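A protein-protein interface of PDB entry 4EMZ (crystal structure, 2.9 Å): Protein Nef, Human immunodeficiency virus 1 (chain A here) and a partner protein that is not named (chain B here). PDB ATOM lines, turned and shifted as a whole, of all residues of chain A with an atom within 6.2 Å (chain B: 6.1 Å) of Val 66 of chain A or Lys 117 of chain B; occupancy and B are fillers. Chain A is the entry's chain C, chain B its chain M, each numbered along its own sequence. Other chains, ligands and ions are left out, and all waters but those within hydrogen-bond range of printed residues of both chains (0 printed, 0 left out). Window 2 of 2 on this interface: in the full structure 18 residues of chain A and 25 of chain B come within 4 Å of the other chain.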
ATOM      1  N   GLU A  63      -5.851   5.782  22.949  1.00  0.00           N
ATOM      2  CA  GLU A  63      -6.584   6.797  23.633  1.00  0.00           C
ATOM      3  C   GLU A  63      -8.036   6.459  23.493  1.00  0.00           C
ATOM      4  O   GLU A  63      -8.588   6.413  22.384  1.00  0.00           O
ATOM      5  CB  GLU A  63      -6.263   8.187  23.120  1.00  0.00           C
ATOM      6  CG  GLU A  63      -5.071   8.785  23.837  1.00  0.00           C
ATOM      7  CD  GLU A  63      -5.182  10.268  24.085  1.00  0.00           C
ATOM      8  OE1 GLU A  63      -4.287  10.765  24.783  1.00  0.00           O
ATOM      9  OE2 GLU A  63      -6.120  10.955  23.607  1.00  0.00           O
ATOM     10  N   GLU A  64      -8.612   6.194  24.658  1.00  0.00           N
ATOM     11  CA  GLU A  64      -9.991   5.749  24.798  1.00  0.00           C
ATOM     12  C   GLU A  64     -10.949   6.922  24.671  1.00  0.00           C
ATOM     13  O   GLU A  64     -10.708   7.986  25.203  1.00  0.00           O
ATOM     14  CB  GLU A  64     -10.200   5.055  26.156  1.00  0.00           C
ATOM     15  CG  GLU A  64      -9.388   5.671  27.314  1.00  0.00           C
ATOM     16  CD  GLU A  64     -10.249   6.062  28.508  1.00  0.00           C
ATOM     17  OE1 GLU A  64     -11.466   5.765  28.517  1.00  0.00           O
ATOM     18  OE2 GLU A  64      -9.715   6.696  29.452  1.00  0.00           O
ATOM     19  N   GLU A  65     -12.040   6.720  23.958  1.00  0.00           N
ATOM     20  CA  GLU A  65     -13.094   7.713  23.930  1.00  0.00           C
ATOM     21  C   GLU A  65     -14.251   7.142  24.703  1.00  0.00           C
ATOM     22  O   GLU A  65     -14.545   5.959  24.585  1.00  0.00           O
ATOM     23  CB  GLU A  65     -13.499   8.060  22.507  1.00  0.00           C
ATOM     24  CG  GLU A  65     -12.386   8.766  21.740  1.00  0.00           C
ATOM     25  CD  GLU A  65     -12.891   9.476  20.481  1.00  0.00           C
ATOM     26  OE1 GLU A  65     -12.247  10.453  20.024  1.00  0.00           O
ATOM     27  OE2 GLU A  65     -13.941   9.055  19.942  1.00  0.00           O
ATOM     28  N   VAL A  66     -14.889   7.977  25.512  1.00  0.00           N
ATOM     29  CA  VAL A  66     -15.885   7.490  26.454  1.00  0.00           C
ATOM     30  C   VAL A  66     -17.233   7.333  25.823  1.00  0.00           C
ATOM     31  O   VAL A  66     -17.597   8.049  24.885  1.00  0.00           O
ATOM     32  CB  VAL A  66     -16.184   8.410  27.629  1.00  0.00           C
ATOM     33  CG1 VAL A  66     -16.351   7.572  28.880  1.00  0.00           C
ATOM     34  CG2 VAL A  66     -15.096   9.439  27.797  1.00  0.00           C
ATOM     35  N   GLY A  67     -17.960   6.374  26.384  1.00  0.00           N
ATOM     36  CA  GLY A  67     -19.353   6.172  26.107  1.00  0.00           C
ATOM     37  C   GLY A  67     -19.738   5.102  25.123  1.00  0.00           C
ATOM     38  O   GLY A  67     -18.942   4.565  24.389  1.00  0.00           O
ATOM     39  N   PHE A  68     -21.032   4.849  25.094  1.00  0.00           N
ATOM     40  CA  PHE A  68     -21.637   3.841  24.268  1.00  0.00           C
ATOM     41  C   PHE A  68     -22.750   4.425  23.370  1.00  0.00           C
ATOM     42  O   PHE A  68     -23.925   4.422  23.746  1.00  0.00           O
ATOM     43  CB  PHE A  68     -22.200   2.759  25.172  1.00  0.00           C
ATOM     44  CG  PHE A  68     -21.158   2.043  26.000  1.00  0.00           C
ATOM     45  CD1 PHE A  68     -20.434   0.991  25.454  1.00  0.00           C
ATOM     46  CD2 PHE A  68     -20.915   2.404  27.327  1.00  0.00           C
ATOM     47  CE1 PHE A  68     -19.495   0.309  26.207  1.00  0.00           C
ATOM     48  CE2 PHE A  68     -19.974   1.734  28.082  1.00  0.00           C
ATOM     49  CZ  PHE A  68     -19.260   0.683  27.525  1.00  0.00           C
ATOM     50  N   PRO A  69     -22.376   4.923  22.179  1.00  0.00           N
ATOM     51  CA  PRO A  69     -23.276   5.469  21.207  1.00  0.00           C
ATOM     52  C   PRO A  69     -24.197   4.429  20.687  1.00  0.00           C
ATOM     53  O   PRO A  69     -23.911   3.252  20.739  1.00  0.00           O
ATOM     54  CB  PRO A  69     -22.369   5.897  20.072  1.00  0.00           C
ATOM     55  CG  PRO A  69     -21.083   6.139  20.705  1.00  0.00           C
ATOM     56  CD  PRO A  69     -20.978   5.126  21.787  1.00  0.00           C
ATOM     57  N   THR B 114     -17.788   5.442  38.467  1.00  0.00           N
ATOM     58  CA  THR B 114     -16.684   5.239  37.567  1.00  0.00           C
ATOM     59  C   THR B 114     -15.631   6.283  37.628  1.00  0.00           C
ATOM     60  O   THR B 114     -15.925   7.457  37.606  1.00  0.00           O
ATOM     61  CB  THR B 114     -17.077   5.363  36.134  1.00  0.00           C
ATOM     62  OG1 THR B 114     -15.875   5.638  35.412  1.00  0.00           O
ATOM     63  CG2 THR B 114     -18.056   6.517  35.979  1.00  0.00           C
ATOM     64  N   HIS B 115     -14.378   5.848  37.601  1.00  0.00           N
ATOM     65  CA  HIS B 115     -13.295   6.718  37.160  1.00  0.00           C
ATOM     66  C   HIS B 115     -13.062   6.401  35.696  1.00  0.00           C
ATOM     67  O   HIS B 115     -12.565   5.339  35.319  1.00  0.00           O
ATOM     68  CB  HIS B 115     -12.025   6.581  38.020  1.00  0.00           C
ATOM     69  CG  HIS B 115     -11.471   7.905  38.527  1.00  0.00           C
ATOM     70  ND1 HIS B 115     -10.583   8.658  37.833  1.00  0.00           N
ATOM     71  CD2 HIS B 115     -11.703   8.580  39.719  1.00  0.00           C
ATOM     72  CE1 HIS B 115     -10.277   9.762  38.546  1.00  0.00           C
ATOM     73  NE2 HIS B 115     -10.968   9.719  39.697  1.00  0.00           N
ATOM     74  N   VAL B 116     -13.473   7.354  34.870  1.00  0.00           N
ATOM     75  CA  VAL B 116     -13.418   7.306  33.395  1.00  0.00           C
ATOM     76  C   VAL B 116     -13.408   8.758  32.933  1.00  0.00           C
ATOM     77  O   VAL B 116     -14.016   9.615  33.601  1.00  0.00           O
ATOM     78  CB  VAL B 116     -14.640   6.609  32.761  1.00  0.00           C
ATOM     79  CG1 VAL B 116     -15.882   7.498  32.872  1.00  0.00           C
ATOM     80  CG2 VAL B 116     -14.364   6.209  31.314  1.00  0.00           C
ATOM     81  N   LYS B 117     -12.756   9.044  31.802  1.00  0.00           N
ATOM     82  CA  LYS B 117     -12.614  10.421  31.375  1.00  0.00           C
ATOM     83  C   LYS B 117     -13.968  11.120  31.501  1.00  0.00           C
ATOM     84  O   LYS B 117     -14.998  10.566  31.081  1.00  0.00           O
ATOM     85  CB  LYS B 117     -12.126  10.524  29.947  1.00  0.00           C
ATOM     86  CG  LYS B 117     -10.759   9.926  29.692  1.00  0.00           C
ATOM     87  CD  LYS B 117     -10.054  10.528  28.484  1.00  0.00           C
ATOM     88  CE  LYS B 117     -10.733  10.046  27.225  1.00  0.00           C
ATOM     89  NZ  LYS B 117     -10.057  10.332  25.937  1.00  0.00           N
ATOM     90  N   PRO B 118     -13.993  12.317  32.115  1.00  0.00           N
ATOM     91  CA  PRO B 118     -15.215  13.084  32.109  1.00  0.00           C
ATOM     92  C   PRO B 118     -15.639  13.405  30.688  1.00  0.00           C
ATOM     93  O   PRO B 118     -14.801  13.539  29.804  1.00  0.00           O
ATOM     94  CB  PRO B 118     -14.818  14.379  32.802  1.00  0.00           C
ATOM     95  CG  PRO B 118     -13.727  13.973  33.709  1.00  0.00           C
ATOM     96  CD  PRO B 118     -12.966  12.954  32.942  1.00  0.00           C
ATOM     97  N   LEU B 119     -16.941  13.496  30.454  1.00  0.00           N
ATOM     98  CA  LEU B 119     -17.427  13.617  29.081  1.00  0.00           C
ATOM     99  C   LEU B 119     -16.937  14.924  28.515  1.00  0.00           C
ATOM    100  O   LEU B 119     -16.399  14.994  27.400  1.00  0.00           O
ATOM    101  CB  LEU B 119     -18.947  13.568  29.024  1.00  0.00           C
ATOM    102  CG  LEU B 119     -19.612  12.230  29.346  1.00  0.00           C
ATOM    103  CD1 LEU B 119     -21.120  12.379  29.371  1.00  0.00           C
ATOM    104  CD2 LEU B 119     -19.233  11.177  28.310  1.00  0.00           C
ATOM    105  N   ILE B 120     -17.129  15.963  29.298  1.00  0.00           N
ATOM    106  CA  ILE B 120     -16.690  17.263  28.899  1.00  0.00           C
ATOM    107  C   ILE B 120     -15.657  17.687  29.900  1.00  0.00           C
ATOM    108  O   ILE B 120     -15.917  17.708  31.104  1.00  0.00           O
ATOM    109  CB  ILE B 120     -17.850  18.248  28.860  1.00  0.00           C
ATOM    110  CG1 ILE B 120     -18.674  17.987  27.587  1.00  0.00           C
ATOM    111  CG2 ILE B 120     -17.354  19.702  28.860  1.00  0.00           C
ATOM    112  CD1 ILE B 120     -20.173  18.099  27.823  1.00  0.00           C
ATOM    113  N   LYS B 141     -13.140  20.671  26.080  1.00  0.00           N
ATOM    114  CA  LYS B 141     -12.761  19.495  25.319  1.00  0.00           C
ATOM    115  C   LYS B 141     -13.789  18.377  25.499  1.00  0.00           C
ATOM    116  O   LYS B 141     -14.125  18.000  26.616  1.00  0.00           O
ATOM    117  CB  LYS B 141     -11.367  19.060  25.773  1.00  0.00           C
ATOM    118  CG  LYS B 141     -10.848  17.738  25.238  1.00  0.00           C
ATOM    119  CD  LYS B 141      -9.647  17.267  26.065  1.00  0.00           C
ATOM    120  CE  LYS B 141      -9.147  15.889  25.657  1.00  0.00           C
ATOM    121  NZ  LYS B 141      -7.981  15.478  26.498  1.00  0.00           N
ATOM    122  N   GLN B 143     -14.727  14.636  25.283  1.00  0.00           N
ATOM    123  CA  GLN B 143     -13.944  13.422  25.394  1.00  0.00           C
ATOM    124  C   GLN B 143     -14.724  12.161  25.034  1.00  0.00           C
ATOM    125  O   GLN B 143     -14.214  11.057  25.137  1.00  0.00           O
ATOM    126  CB  GLN B 143     -13.392  13.322  26.813  1.00  0.00           C
ATOM    127  CG  GLN B 143     -12.379  14.420  27.166  1.00  0.00           C
ATOM    128  CD  GLN B 143     -11.461  14.008  28.311  1.00  0.00           C
ATOM    129  OE1 GLN B 143     -10.264  13.812  28.125  1.00  0.00           O
ATOM    130  NE2 GLN B 143     -12.032  13.866  29.502  1.00  0.00           N
ATOM    131  N   PHE B 144     -15.984  12.326  24.654  1.00  0.00           N
ATOM    132  CA  PHE B 144     -16.831  11.174  24.271  1.00  0.00           C
ATOM    133  C   PHE B 144     -16.663  10.918  22.803  1.00  0.00           C
ATOM    134  O   PHE B 144     -16.028  11.695  22.101  1.00  0.00           O
ATOM    135  CB  PHE B 144     -18.317  11.418  24.575  1.00  0.00           C
ATOM    136  CG  PHE B 144     -18.822  12.759  24.100  1.00  0.00           C
ATOM    137  CD1 PHE B 144     -19.209  12.933  22.788  1.00  0.00           C
ATOM    138  CD2 PHE B 144     -18.879  13.864  24.972  1.00  0.00           C
ATOM    139  CE1 PHE B 144     -19.648  14.175  22.356  1.00  0.00           C
ATOM    140  CE2 PHE B 144     -19.308  15.102  24.532  1.00  0.00           C
ATOM    141  CZ  PHE B 144     -19.696  15.265  23.226  1.00  0.00           C
ATOM    142  N   LYS B 145     -17.257   9.829  22.344  1.00  0.00           N
ATOM    143  CA  LYS B 145     -17.089   9.335  20.958  1.00  0.00           C
ATOM    144  C   LYS B 145     -17.334  10.386  19.858  1.00  0.00           C
ATOM    145  O   LYS B 145     -18.215  11.209  19.956  1.00  0.00           O
ATOM    146  CB  LYS B 145     -17.985   8.130  20.744  1.00  0.00           C
ATOM    147  CG  LYS B 145     -17.620   6.950  21.634  1.00  0.00           C
ATOM    148  CD  LYS B 145     -16.435   6.173  21.078  1.00  0.00           C
ATOM    149  CE  LYS B 145     -15.851   5.181  22.076  1.00  0.00           C
ATOM    150  NZ  LYS B 145     -16.816   4.174  22.596  1.00  0.00           N
ATOM    151  N   PHE B 228     -27.094   8.012  23.273  1.00  0.00           N
ATOM    152  CA  PHE B 228     -25.853   7.804  24.078  1.00  0.00           C
ATOM    153  C   PHE B 228     -26.097   7.296  25.505  1.00  0.00           C
ATOM    154  O   PHE B 228     -27.094   7.612  26.122  1.00  0.00           O
ATOM    155  CB  PHE B 228     -25.108   9.133  24.204  1.00  0.00           C
ATOM    156  CG  PHE B 228     -23.682   9.023  24.697  1.00  0.00           C
ATOM    157  CD1 PHE B 228     -22.632   8.781  23.811  1.00  0.00           C
ATOM    158  CD2 PHE B 228     -23.379   9.272  26.020  1.00  0.00           C
ATOM    159  CE1 PHE B 228     -21.327   8.728  24.265  1.00  0.00           C
ATOM    160  CE2 PHE B 228     -22.066   9.252  26.489  1.00  0.00           C
ATOM    161  CZ  PHE B 228     -21.045   8.988  25.608  1.00  0.00           C
ATOM    162  N   THR B 229     -25.152   6.534  26.030  1.00  0.00           N
ATOM    163  CA  THR B 229     -25.052   6.313  27.488  1.00  0.00           C
ATOM    164  C   THR B 229     -23.601   6.160  27.870  1.00  0.00           C
ATOM    165  O   THR B 229     -22.776   5.782  27.052  1.00  0.00           O
ATOM    166  CB  THR B 229     -25.872   5.111  28.079  1.00  0.00           C
ATOM    167  OG1 THR B 229     -25.280   3.842  27.796  1.00  0.00           O
ATOM    168  CG2 THR B 229     -27.241   5.117  27.561  1.00  0.00           C
ATOM    169  N   THR B 230     -23.292   6.470  29.115  1.00  0.00           N
ATOM    170  CA  THR B 230     -21.937   6.277  29.586  1.00  0.00           C
ATOM    171  C   THR B 230     -21.791   4.919  30.239  1.00  0.00           C
ATOM    172  O   THR B 230     -20.671   4.446  30.402  1.00  0.00           O
ATOM    173  CB  THR B 230     -21.438   7.400  30.506  1.00  0.00           C
ATOM    174  OG1 THR B 230     -22.525   8.196  30.997  1.00  0.00           O
ATOM    175  CG2 THR B 230     -20.563   8.313  29.734  1.00  0.00           C
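O of Glu 64 of chain A lies within hydrogen-bond range of NZ of Lys 117 of chain B, 2.5 Å away.
N of Val 66 of chain A is in hydrogen-bond range of O of Gln 143 of chain B, at 3.2 Å.
O of Val 66 of chain A is in hydrogen-bond range of N of Lys 145 of chain B, 3.1 Å away.
The side-chain amino group of Lys 145 of chain B lies within hydrogen-bond range of the backbone carbonyl oxygen of Gly 67 of chain A, 2.8 Å away.
The backbone NH (N) of Phe 68 of chain A is in hydrogen-bond range of the backbone carbonyl oxygen (O) of Thr 229 of chain B (2.8 Å).
The backbone NH of Val 116 of chain B lies within hydrogen-bond range of the side-chain hydroxyl of Thr 114 of chain B (3.0 Å).
NE2 of Gln 143 of chain B lies within hydrogen-bond range of O of Pro 118 of chain B (2.8 Å).
The backbone carbonyl oxygen (O) of Leu 119 of chain B sits at hydrogen-bond distance from the backbone NH (N) of Gln 143 of chain B, at 2.7 Å.
NZ of Lys 141 of chain B lies within hydrogen-bond range of OE1 of Gln 143 of chain B, 3.3 Å away.
Among the printed residues, pairs that only touch across the chains: Glu 65 of chain A with Lys 145 of chain B, Val 66 of chain A with Phe 144 of chain B, Gly 67 of chain A with Phe 228 of chain B, Val 66 of chain A with Val 116 of chain B, Val 66 of chain A with Lys 117 of chain B, Gly 67 of chain A with Thr 229 of chain B, Phe 68 of chain A with Thr 230 of chain B, Val 66 of chain A with Phe 228 of chain B, Pro 69 of chain A with Lys 145 of chain B, Glu 65 of chain A with Gln 143 of chain B, Phe 68 of chain A with Phe 228 of chain B and Glu 65 of chain A with Phe 144 of chain B.
Val 66 of chain A touches just these residues of chain B: Val 116, Lys 117, Gln 143, Phe 144, Lys 145 and Phe 228.
Lys 117 of chain B touches two residues of chain A.
Printed residues of chain A within 4 Å of Thr 229 of chain B: Gly 67 (3.6 Å) and Phe 68 (2.8 Å).
Printed residues of chain B within 4 Å of Glu 64 of chain A: Lys 117 (2.5 Å).
Pro 118 of chain B touches none of the printed residues of chain A.
His 115 of chain B touches none of the printed residues of chain A.
The nearest printed residue of chain B that does not touch Phe 68 of chain A is Lys 145 of chain B (4.9 Å).
Of the 14 printed residues of chain B, 8 touch a printed residue of chain A.
Of the 7 printed residues of chain A, 6 touch a printed residue of chain B.
Among the printed residues, no Asp or Glu carboxylate lies within 4 Å of a Lys or Arg side-chain nitrogen of the other chain.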
